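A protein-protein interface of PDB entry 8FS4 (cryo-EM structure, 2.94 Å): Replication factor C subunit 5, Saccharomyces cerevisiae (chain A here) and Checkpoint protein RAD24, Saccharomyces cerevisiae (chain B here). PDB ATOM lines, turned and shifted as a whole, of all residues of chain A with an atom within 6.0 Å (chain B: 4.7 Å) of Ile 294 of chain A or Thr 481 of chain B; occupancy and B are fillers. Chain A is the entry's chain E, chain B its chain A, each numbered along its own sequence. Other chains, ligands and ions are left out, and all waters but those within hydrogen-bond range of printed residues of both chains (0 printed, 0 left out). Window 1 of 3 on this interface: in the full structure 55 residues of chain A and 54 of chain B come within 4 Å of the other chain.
O of Leu 482 of chain B sits at hydrogen-bond distance from NE1 of Trp 259 of chain A (3.0 Å).
The side-chain hydroxyl (OG1) of Thr 481 of chain B sits at hydrogen-bond distance from the backbone carbonyl oxygen (O) of Arg 478 of chain B, at 2.8 Å.
The side-chain hydroxyl (OG1) of Thr 481 of chain B sits close to the backbone carbonyl oxygen (O) of Phe 477 of chain B.
Trp 259 of chain A touches Ile 543 of chain B (N to CD1, 3.4 Å).
O of His 292 of chain A touches CE2 of Phe 456 of chain B, 3.2 Å away.
CA of Ile 543 of chain B touches NE2 of His 292 of chain A, at 3.3 Å.
SG of Cys 293 of chain A touches CD1 of Phe 456 of chain B, at 3.5 Å.
Phe 477 of chain B touches Cys 293 of chain A.
Cys 293 of chain A touches Thr 481 of chain B.
Ile 294 of chain A touches Thr 481 of chain B.
Pro 295 of chain A touches Arg 478 of chain B.
Pro 295 of chain A touches Leu 482 of chain B.
CD1 of Ile 298 of chain A touches NH2 of Arg 478 of chain B, 3.3 Å away.
Ile 294 of chain A touches one residue of chain B.
Thr 481 of chain B touches two residues of chain A.
Printed residues of chain A within 4 Å of Ile 543 of chain B: Trp 259 (3.4 Å) and His 292 (3.3 Å).
Of the printed residues of chain B, Cys 293 of chain A touches Phe 456 (3.5 Å), Phe 477 (3.7 Å) and Thr 481 (3.7 Å).
Printed residues of chain B within 4 Å of Trp 259 of chain A: Leu 482 (3.0 Å) and Ile 543 (3.4 Å).
Of the printed residues of chain B, His 292 of chain A touches Phe 456 and Ile 543.
Of the printed residues of chain A, Arg 478 of chain B touches Pro 295 and Ile 298.
Glu 483 of chain B touches none of the printed residues of chain A.
The nearest printed residue of chain B that does not touch Ile 294 of chain A is Arg 538 of chain B (4.7 Å).
The nearest residue of chain A that does not touch Thr 481 of chain B is His 292 of chain A (4.2 Å).
The nearest printed residue of chain B that does not touch Trp 259 of chain A is Arg 538 of chain B (4.9 Å).
Of the 11 printed residues of chain A, 6 touch a printed residue of chain B.
Hydrophobic or aromatic side chains of chain A within 4 Å of the printed part of chain B: Trp 259, His 292, Ile 294, Pro 295 and Ile 298.
Among the printed residues, no Asp or Glu carboxylate lies within 4 Å of a Lys or Arg side-chain nitrogen of the other chain.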
ATOM      1  N   TRP A 259      16.294 -11.478  29.607  1.00  0.00           N
ATOM      2  CA  TRP A 259      17.135 -11.264  28.438  1.00  0.00           C
ATOM      3  C   TRP A 259      18.014 -12.478  28.158  1.00  0.00           C
ATOM      4  O   TRP A 259      18.328 -12.756  26.998  1.00  0.00           O
ATOM      5  CB  TRP A 259      17.975  -9.999  28.613  1.00  0.00           C
ATOM      6  CG  TRP A 259      18.966 -10.050  29.723  1.00  0.00           C
ATOM      7  CD1 TRP A 259      18.722  -9.874  31.049  1.00  0.00           C
ATOM      8  CD2 TRP A 259      20.372 -10.280  29.600  1.00  0.00           C
ATOM      9  NE1 TRP A 259      19.888  -9.986  31.764  1.00  0.00           N
ATOM     10  CE2 TRP A 259      20.917 -10.236  30.895  1.00  0.00           C
ATOM     11  CE3 TRP A 259      21.222 -10.522  28.519  1.00  0.00           C
ATOM     12  CZ2 TRP A 259      22.270 -10.426  31.140  1.00  0.00           C
ATOM     13  CZ3 TRP A 259      22.564 -10.709  28.763  1.00  0.00           C
ATOM     14  CH2 TRP A 259      23.077 -10.661  30.063  1.00  0.00           C
ATOM     15  N   LEU A 289      16.121  -6.214  22.393  1.00  0.00           N
ATOM     16  CA  LEU A 289      17.069  -6.304  23.500  1.00  0.00           C
ATOM     17  C   LEU A 289      17.761  -4.971  23.744  1.00  0.00           C
ATOM     18  O   LEU A 289      17.889  -4.528  24.891  1.00  0.00           O
ATOM     19  CB  LEU A 289      18.104  -7.395  23.221  1.00  0.00           C
ATOM     20  CG  LEU A 289      17.640  -8.838  23.420  1.00  0.00           C
ATOM     21  CD1 LEU A 289      18.639  -9.809  22.821  1.00  0.00           C
ATOM     22  CD2 LEU A 289      17.424  -9.138  24.891  1.00  0.00           C
ATOM     23  N   LEU A 290      18.215  -4.311  22.676  1.00  0.00           N
ATOM     24  CA  LEU A 290      18.895  -3.030  22.822  1.00  0.00           C
ATOM     25  C   LEU A 290      17.962  -1.943  23.330  1.00  0.00           C
ATOM     26  O   LEU A 290      18.430  -0.978  23.942  1.00  0.00           O
ATOM     27  CB  LEU A 290      19.507  -2.603  21.488  1.00  0.00           C
ATOM     28  CG  LEU A 290      20.814  -3.291  21.087  1.00  0.00           C
ATOM     29  CD1 LEU A 290      21.171  -2.949  19.653  1.00  0.00           C
ATOM     30  CD2 LEU A 290      21.949  -2.905  22.022  1.00  0.00           C
ATOM     31  N   ALA A 291      16.657  -2.074  23.089  1.00  0.00           N
ATOM     32  CA  ALA A 291      15.702  -1.105  23.608  1.00  0.00           C
ATOM     33  C   ALA A 291      15.643  -1.115  25.129  1.00  0.00           C
ATOM     34  O   ALA A 291      15.109  -0.171  25.720  1.00  0.00           O
ATOM     35  CB  ALA A 291      14.313  -1.381  23.034  1.00  0.00           C
ATOM     36  N   HIS A 292      16.171  -2.157  25.770  1.00  0.00           N
ATOM     37  CA  HIS A 292      16.220  -2.248  27.221  1.00  0.00           C
ATOM     38  C   HIS A 292      17.552  -1.780  27.790  1.00  0.00           C
ATOM     39  O   HIS A 292      17.882  -2.116  28.932  1.00  0.00           O
ATOM     40  CB  HIS A 292      15.933  -3.683  27.664  1.00  0.00           C
ATOM     41  CG  HIS A 292      14.528  -4.123  27.399  1.00  0.00           C
ATOM     42  ND1 HIS A 292      13.446  -3.598  28.073  1.00  0.00           N
ATOM     43  CD2 HIS A 292      14.027  -5.030  26.529  1.00  0.00           C
ATOM     44  CE1 HIS A 292      12.339  -4.167  27.631  1.00  0.00           C
ATOM     45  NE2 HIS A 292      12.664  -5.039  26.695  1.00  0.00           N
ATOM     46  N   CYS A 293      18.326  -1.020  27.018  1.00  0.00           N
ATOM     47  CA  CYS A 293      19.594  -0.453  27.465  1.00  0.00           C
ATOM     48  C   CYS A 293      20.601  -1.524  27.863  1.00  0.00           C
ATOM     49  O   CYS A 293      21.499  -1.265  28.667  1.00  0.00           O
ATOM     50  CB  CYS A 293      19.384   0.521  28.627  1.00  0.00           C
ATOM     51  SG  CYS A 293      18.409   1.979  28.205  1.00  0.00           S
ATOM     52  N   ILE A 294      20.473  -2.727  27.322  1.00  0.00           N
ATOM     53  CA  ILE A 294      21.452  -3.779  27.595  1.00  0.00           C
ATOM     54  C   ILE A 294      22.679  -3.543  26.717  1.00  0.00           C
ATOM     55  O   ILE A 294      22.537  -3.427  25.491  1.00  0.00           O
ATOM     56  CB  ILE A 294      20.847  -5.157  27.345  1.00  0.00           C
ATOM     57  CG1 ILE A 294      19.830  -5.484  28.438  1.00  0.00           C
ATOM     58  CG2 ILE A 294      21.921  -6.230  27.335  1.00  0.00           C
ATOM     59  CD1 ILE A 294      18.692  -6.352  27.976  1.00  0.00           C
ATOM     60  N   PRO A 295      23.881  -3.461  27.289  1.00  0.00           N
ATOM     61  CA  PRO A 295      25.066  -3.170  26.472  1.00  0.00           C
ATOM     62  C   PRO A 295      25.272  -4.214  25.387  1.00  0.00           C
ATOM     63  O   PRO A 295      25.002  -5.400  25.580  1.00  0.00           O
ATOM     64  CB  PRO A 295      26.212  -3.178  27.491  1.00  0.00           C
ATOM     65  CG  PRO A 295      25.690  -3.919  28.664  1.00  0.00           C
ATOM     66  CD  PRO A 295      24.225  -3.664  28.703  1.00  0.00           C
ATOM     67  N   ALA A 296      25.768  -3.759  24.234  1.00  0.00           N
ATOM     68  CA  ALA A 296      25.883  -4.638  23.076  1.00  0.00           C
ATOM     69  C   ALA A 296      27.010  -5.651  23.232  1.00  0.00           C
ATOM     70  O   ALA A 296      26.905  -6.770  22.718  1.00  0.00           O
ATOM     71  CB  ALA A 296      26.092  -3.809  21.812  1.00  0.00           C
ATOM     72  N   ILE A 298      27.851  -7.176  25.973  1.00  0.00           N
ATOM     73  CA  ILE A 298      27.280  -8.264  26.762  1.00  0.00           C
ATOM     74  C   ILE A 298      26.362  -9.121  25.901  1.00  0.00           C
ATOM     75  O   ILE A 298      26.353 -10.353  26.017  1.00  0.00           O
ATOM     76  CB  ILE A 298      26.544  -7.699  27.993  1.00  0.00           C
ATOM     77  CG1 ILE A 298      27.529  -7.062  28.985  1.00  0.00           C
ATOM     78  CG2 ILE A 298      25.740  -8.787  28.692  1.00  0.00           C
ATOM     79  CD1 ILE A 298      28.839  -7.816  29.172  1.00  0.00           C
ATOM     80  N   ILE A 299      25.567  -8.490  25.034  1.00  0.00           N
ATOM     81  CA  ILE A 299      24.702  -9.255  24.140  1.00  0.00           C
ATOM     82  C   ILE A 299      25.541 -10.192  23.282  1.00  0.00           C
ATOM     83  O   ILE A 299      25.228 -11.378  23.138  1.00  0.00           O
ATOM     84  CB  ILE A 299      23.849  -8.311  23.274  1.00  0.00           C
ATOM     85  CG1 ILE A 299      22.897  -7.505  24.159  1.00  0.00           C
ATOM     86  CG2 ILE A 299      23.075  -9.103  22.220  1.00  0.00           C
ATOM     87  CD1 ILE A 299      21.826  -6.740  23.407  1.00  0.00           C
ATOM     88  N   PHE B 456      13.466   3.643  29.068  1.00  0.00           N
ATOM     89  CA  PHE B 456      14.074   2.719  30.021  1.00  0.00           C
ATOM     90  C   PHE B 456      14.935   3.466  31.032  1.00  0.00           C
ATOM     91  O   PHE B 456      14.925   3.149  32.227  1.00  0.00           O
ATOM     92  CB  PHE B 456      14.903   1.678  29.265  1.00  0.00           C
ATOM     93  CG  PHE B 456      15.471   0.591  30.136  1.00  0.00           C
ATOM     94  CD1 PHE B 456      16.562   0.832  30.950  1.00  0.00           C
ATOM     95  CD2 PHE B 456      14.925  -0.680  30.120  1.00  0.00           C
ATOM     96  CE1 PHE B 456      17.083  -0.167  31.745  1.00  0.00           C
ATOM     97  CE2 PHE B 456      15.444  -1.682  30.912  1.00  0.00           C
ATOM     98  CZ  PHE B 456      16.525  -1.426  31.725  1.00  0.00           C
ATOM     99  N   PHE B 477      23.700   1.722  37.029  1.00  0.00           N
ATOM    100  CA  PHE B 477      22.710   1.509  35.981  1.00  0.00           C
ATOM    101  C   PHE B 477      22.978   0.225  35.209  1.00  0.00           C
ATOM    102  O   PHE B 477      22.045  -0.381  34.674  1.00  0.00           O
ATOM    103  CB  PHE B 477      22.685   2.702  35.028  1.00  0.00           C
ATOM    104  CG  PHE B 477      21.688   2.564  33.914  1.00  0.00           C
ATOM    105  CD1 PHE B 477      20.345   2.364  34.188  1.00  0.00           C
ATOM    106  CD2 PHE B 477      22.092   2.632  32.593  1.00  0.00           C
ATOM    107  CE1 PHE B 477      19.428   2.237  33.166  1.00  0.00           C
ATOM    108  CE2 PHE B 477      21.179   2.504  31.567  1.00  0.00           C
ATOM    109  CZ  PHE B 477      19.846   2.309  31.854  1.00  0.00           C
ATOM    110  N   ARG B 478      24.239  -0.200  35.127  1.00  0.00           N
ATOM    111  CA  ARG B 478      24.543  -1.463  34.464  1.00  0.00           C
ATOM    112  C   ARG B 478      23.864  -2.628  35.176  1.00  0.00           C
ATOM    113  O   ARG B 478      23.240  -3.484  34.536  1.00  0.00           O
ATOM    114  CB  ARG B 478      26.057  -1.667  34.414  1.00  0.00           C
ATOM    115  CG  ARG B 478      26.517  -2.780  33.491  1.00  0.00           C
ATOM    116  CD  ARG B 478      27.666  -2.313  32.612  1.00  0.00           C
ATOM    117  NE  ARG B 478      28.125  -3.357  31.703  1.00  0.00           N
ATOM    118  CZ  ARG B 478      28.952  -4.337  32.040  1.00  0.00           C
ATOM    119  NH1 ARG B 478      29.432  -4.449  33.268  1.00  0.00           N
ATOM    120  NH2 ARG B 478      29.308  -5.229  31.120  1.00  0.00           N
ATOM    121  N   ASN B 479      23.959  -2.666  36.504  1.00  0.00           N
ATOM    122  CA  ASN B 479      23.290  -3.722  37.252  1.00  0.00           C
ATOM    123  C   ASN B 479      21.779  -3.571  37.190  1.00  0.00           C
ATOM    124  O   ASN B 479      21.057  -4.567  37.278  1.00  0.00           O
ATOM    125  CB  ASN B 479      23.773  -3.722  38.698  1.00  0.00           C
ATOM    126  CG  ASN B 479      25.270  -3.892  38.806  1.00  0.00           C
ATOM    127  OD1 ASN B 479      25.968  -3.981  37.797  1.00  0.00           O
ATOM    128  ND2 ASN B 479      25.775  -3.940  40.030  1.00  0.00           N
ATOM    129  N   ILE B 480      21.281  -2.346  37.029  1.00  0.00           N
ATOM    130  CA  ILE B 480      19.844  -2.167  36.863  1.00  0.00           C
ATOM    131  C   ILE B 480      19.389  -2.730  35.525  1.00  0.00           C
ATOM    132  O   ILE B 480      18.293  -3.293  35.420  1.00  0.00           O
ATOM    133  CB  ILE B 480      19.477  -0.680  37.018  1.00  0.00           C
ATOM    134  CG1 ILE B 480      19.212  -0.363  38.489  1.00  0.00           C
ATOM    135  CG2 ILE B 480      18.250  -0.325  36.195  1.00  0.00           C
ATOM    136  CD1 ILE B 480      19.424   1.086  38.848  1.00  0.00           C
ATOM    137  N   THR B 481      20.207  -2.587  34.488  1.00  0.00           N
ATOM    138  CA  THR B 481      19.853  -3.037  33.150  1.00  0.00           C
ATOM    139  C   THR B 481      20.110  -4.520  32.934  1.00  0.00           C
ATOM    140  O   THR B 481      19.581  -5.086  31.972  1.00  0.00           O
ATOM    141  CB  THR B 481      20.636  -2.246  32.098  1.00  0.00           C
ATOM    142  OG1 THR B 481      22.040  -2.475  32.265  1.00  0.00           O
ATOM    143  CG2 THR B 481      20.354  -0.764  32.223  1.00  0.00           C
ATOM    144  N   LEU B 482      20.913  -5.155  33.786  1.00  0.00           N
ATOM    145  CA  LEU B 482      21.221  -6.566  33.611  1.00  0.00           C
ATOM    146  C   LEU B 482      20.615  -7.474  34.674  1.00  0.00           C
ATOM    147  O   LEU B 482      20.298  -8.625  34.359  1.00  0.00           O
ATOM    148  CB  LEU B 482      22.744  -6.772  33.565  1.00  0.00           C
ATOM    149  CG  LEU B 482      23.376  -6.515  32.192  1.00  0.00           C
ATOM    150  CD1 LEU B 482      23.269  -5.055  31.813  1.00  0.00           C
ATOM    151  CD2 LEU B 482      24.829  -6.950  32.157  1.00  0.00           C
ATOM    152  N   GLU B 483      20.467  -7.015  35.918  1.00  0.00           N
ATOM    153  CA  GLU B 483      19.927  -7.860  36.978  1.00  0.00           C
ATOM    154  C   GLU B 483      18.675  -7.295  37.643  1.00  0.00           C
ATOM    155  O   GLU B 483      17.636  -7.962  37.676  1.00  0.00           O
ATOM    156  CB  GLU B 483      21.012  -8.102  38.025  1.00  0.00           C
ATOM    157  CG  GLU B 483      22.287  -8.683  37.430  1.00  0.00           C
ATOM    158  CD  GLU B 483      23.518  -8.334  38.225  1.00  0.00           C
ATOM    159  OE1 GLU B 483      23.365  -7.838  39.358  1.00  0.00           O
ATOM    160  OE2 GLU B 483      24.640  -8.552  37.723  1.00  0.00           O
ATOM    161  N   ARG B 538       8.821  -4.657  35.205  1.00  0.00           N
ATOM    162  CA  ARG B 538      10.174  -4.654  34.665  1.00  0.00           C
ATOM    163  C   ARG B 538      10.578  -3.245  34.257  1.00  0.00           C
ATOM    164  O   ARG B 538       9.883  -2.586  33.479  1.00  0.00           O
ATOM    165  CB  ARG B 538      10.267  -5.599  33.465  1.00  0.00           C
ATOM    166  CG  ARG B 538      11.646  -6.227  33.285  1.00  0.00           C
ATOM    167  CD  ARG B 538      11.944  -6.534  31.825  1.00  0.00           C
ATOM    168  NE  ARG B 538      13.361  -6.762  31.565  1.00  0.00           N
ATOM    169  CZ  ARG B 538      14.314  -5.849  31.708  1.00  0.00           C
ATOM    170  NH1 ARG B 538      14.042  -4.618  32.111  1.00  0.00           N
ATOM    171  NH2 ARG B 538      15.574  -6.178  31.434  1.00  0.00           N
ATOM    172  N   ILE B 543      10.566  -7.636  28.053  1.00  0.00           N
ATOM    173  CA  ILE B 543      11.295  -8.074  26.869  1.00  0.00           C
ATOM    174  C   ILE B 543      10.376  -8.949  26.031  1.00  0.00           C
ATOM    175  O   ILE B 543       9.777  -9.904  26.539  1.00  0.00           O
ATOM    176  CB  ILE B 543      12.576  -8.831  27.254  1.00  0.00           C
ATOM    177  CG1 ILE B 543      13.316  -8.098  28.377  1.00  0.00           C
ATOM    178  CG2 ILE B 543      13.477  -8.997  26.033  1.00  0.00           C
ATOM    179  CD1 ILE B 543      14.692  -8.657  28.683  1.00  0.00           C
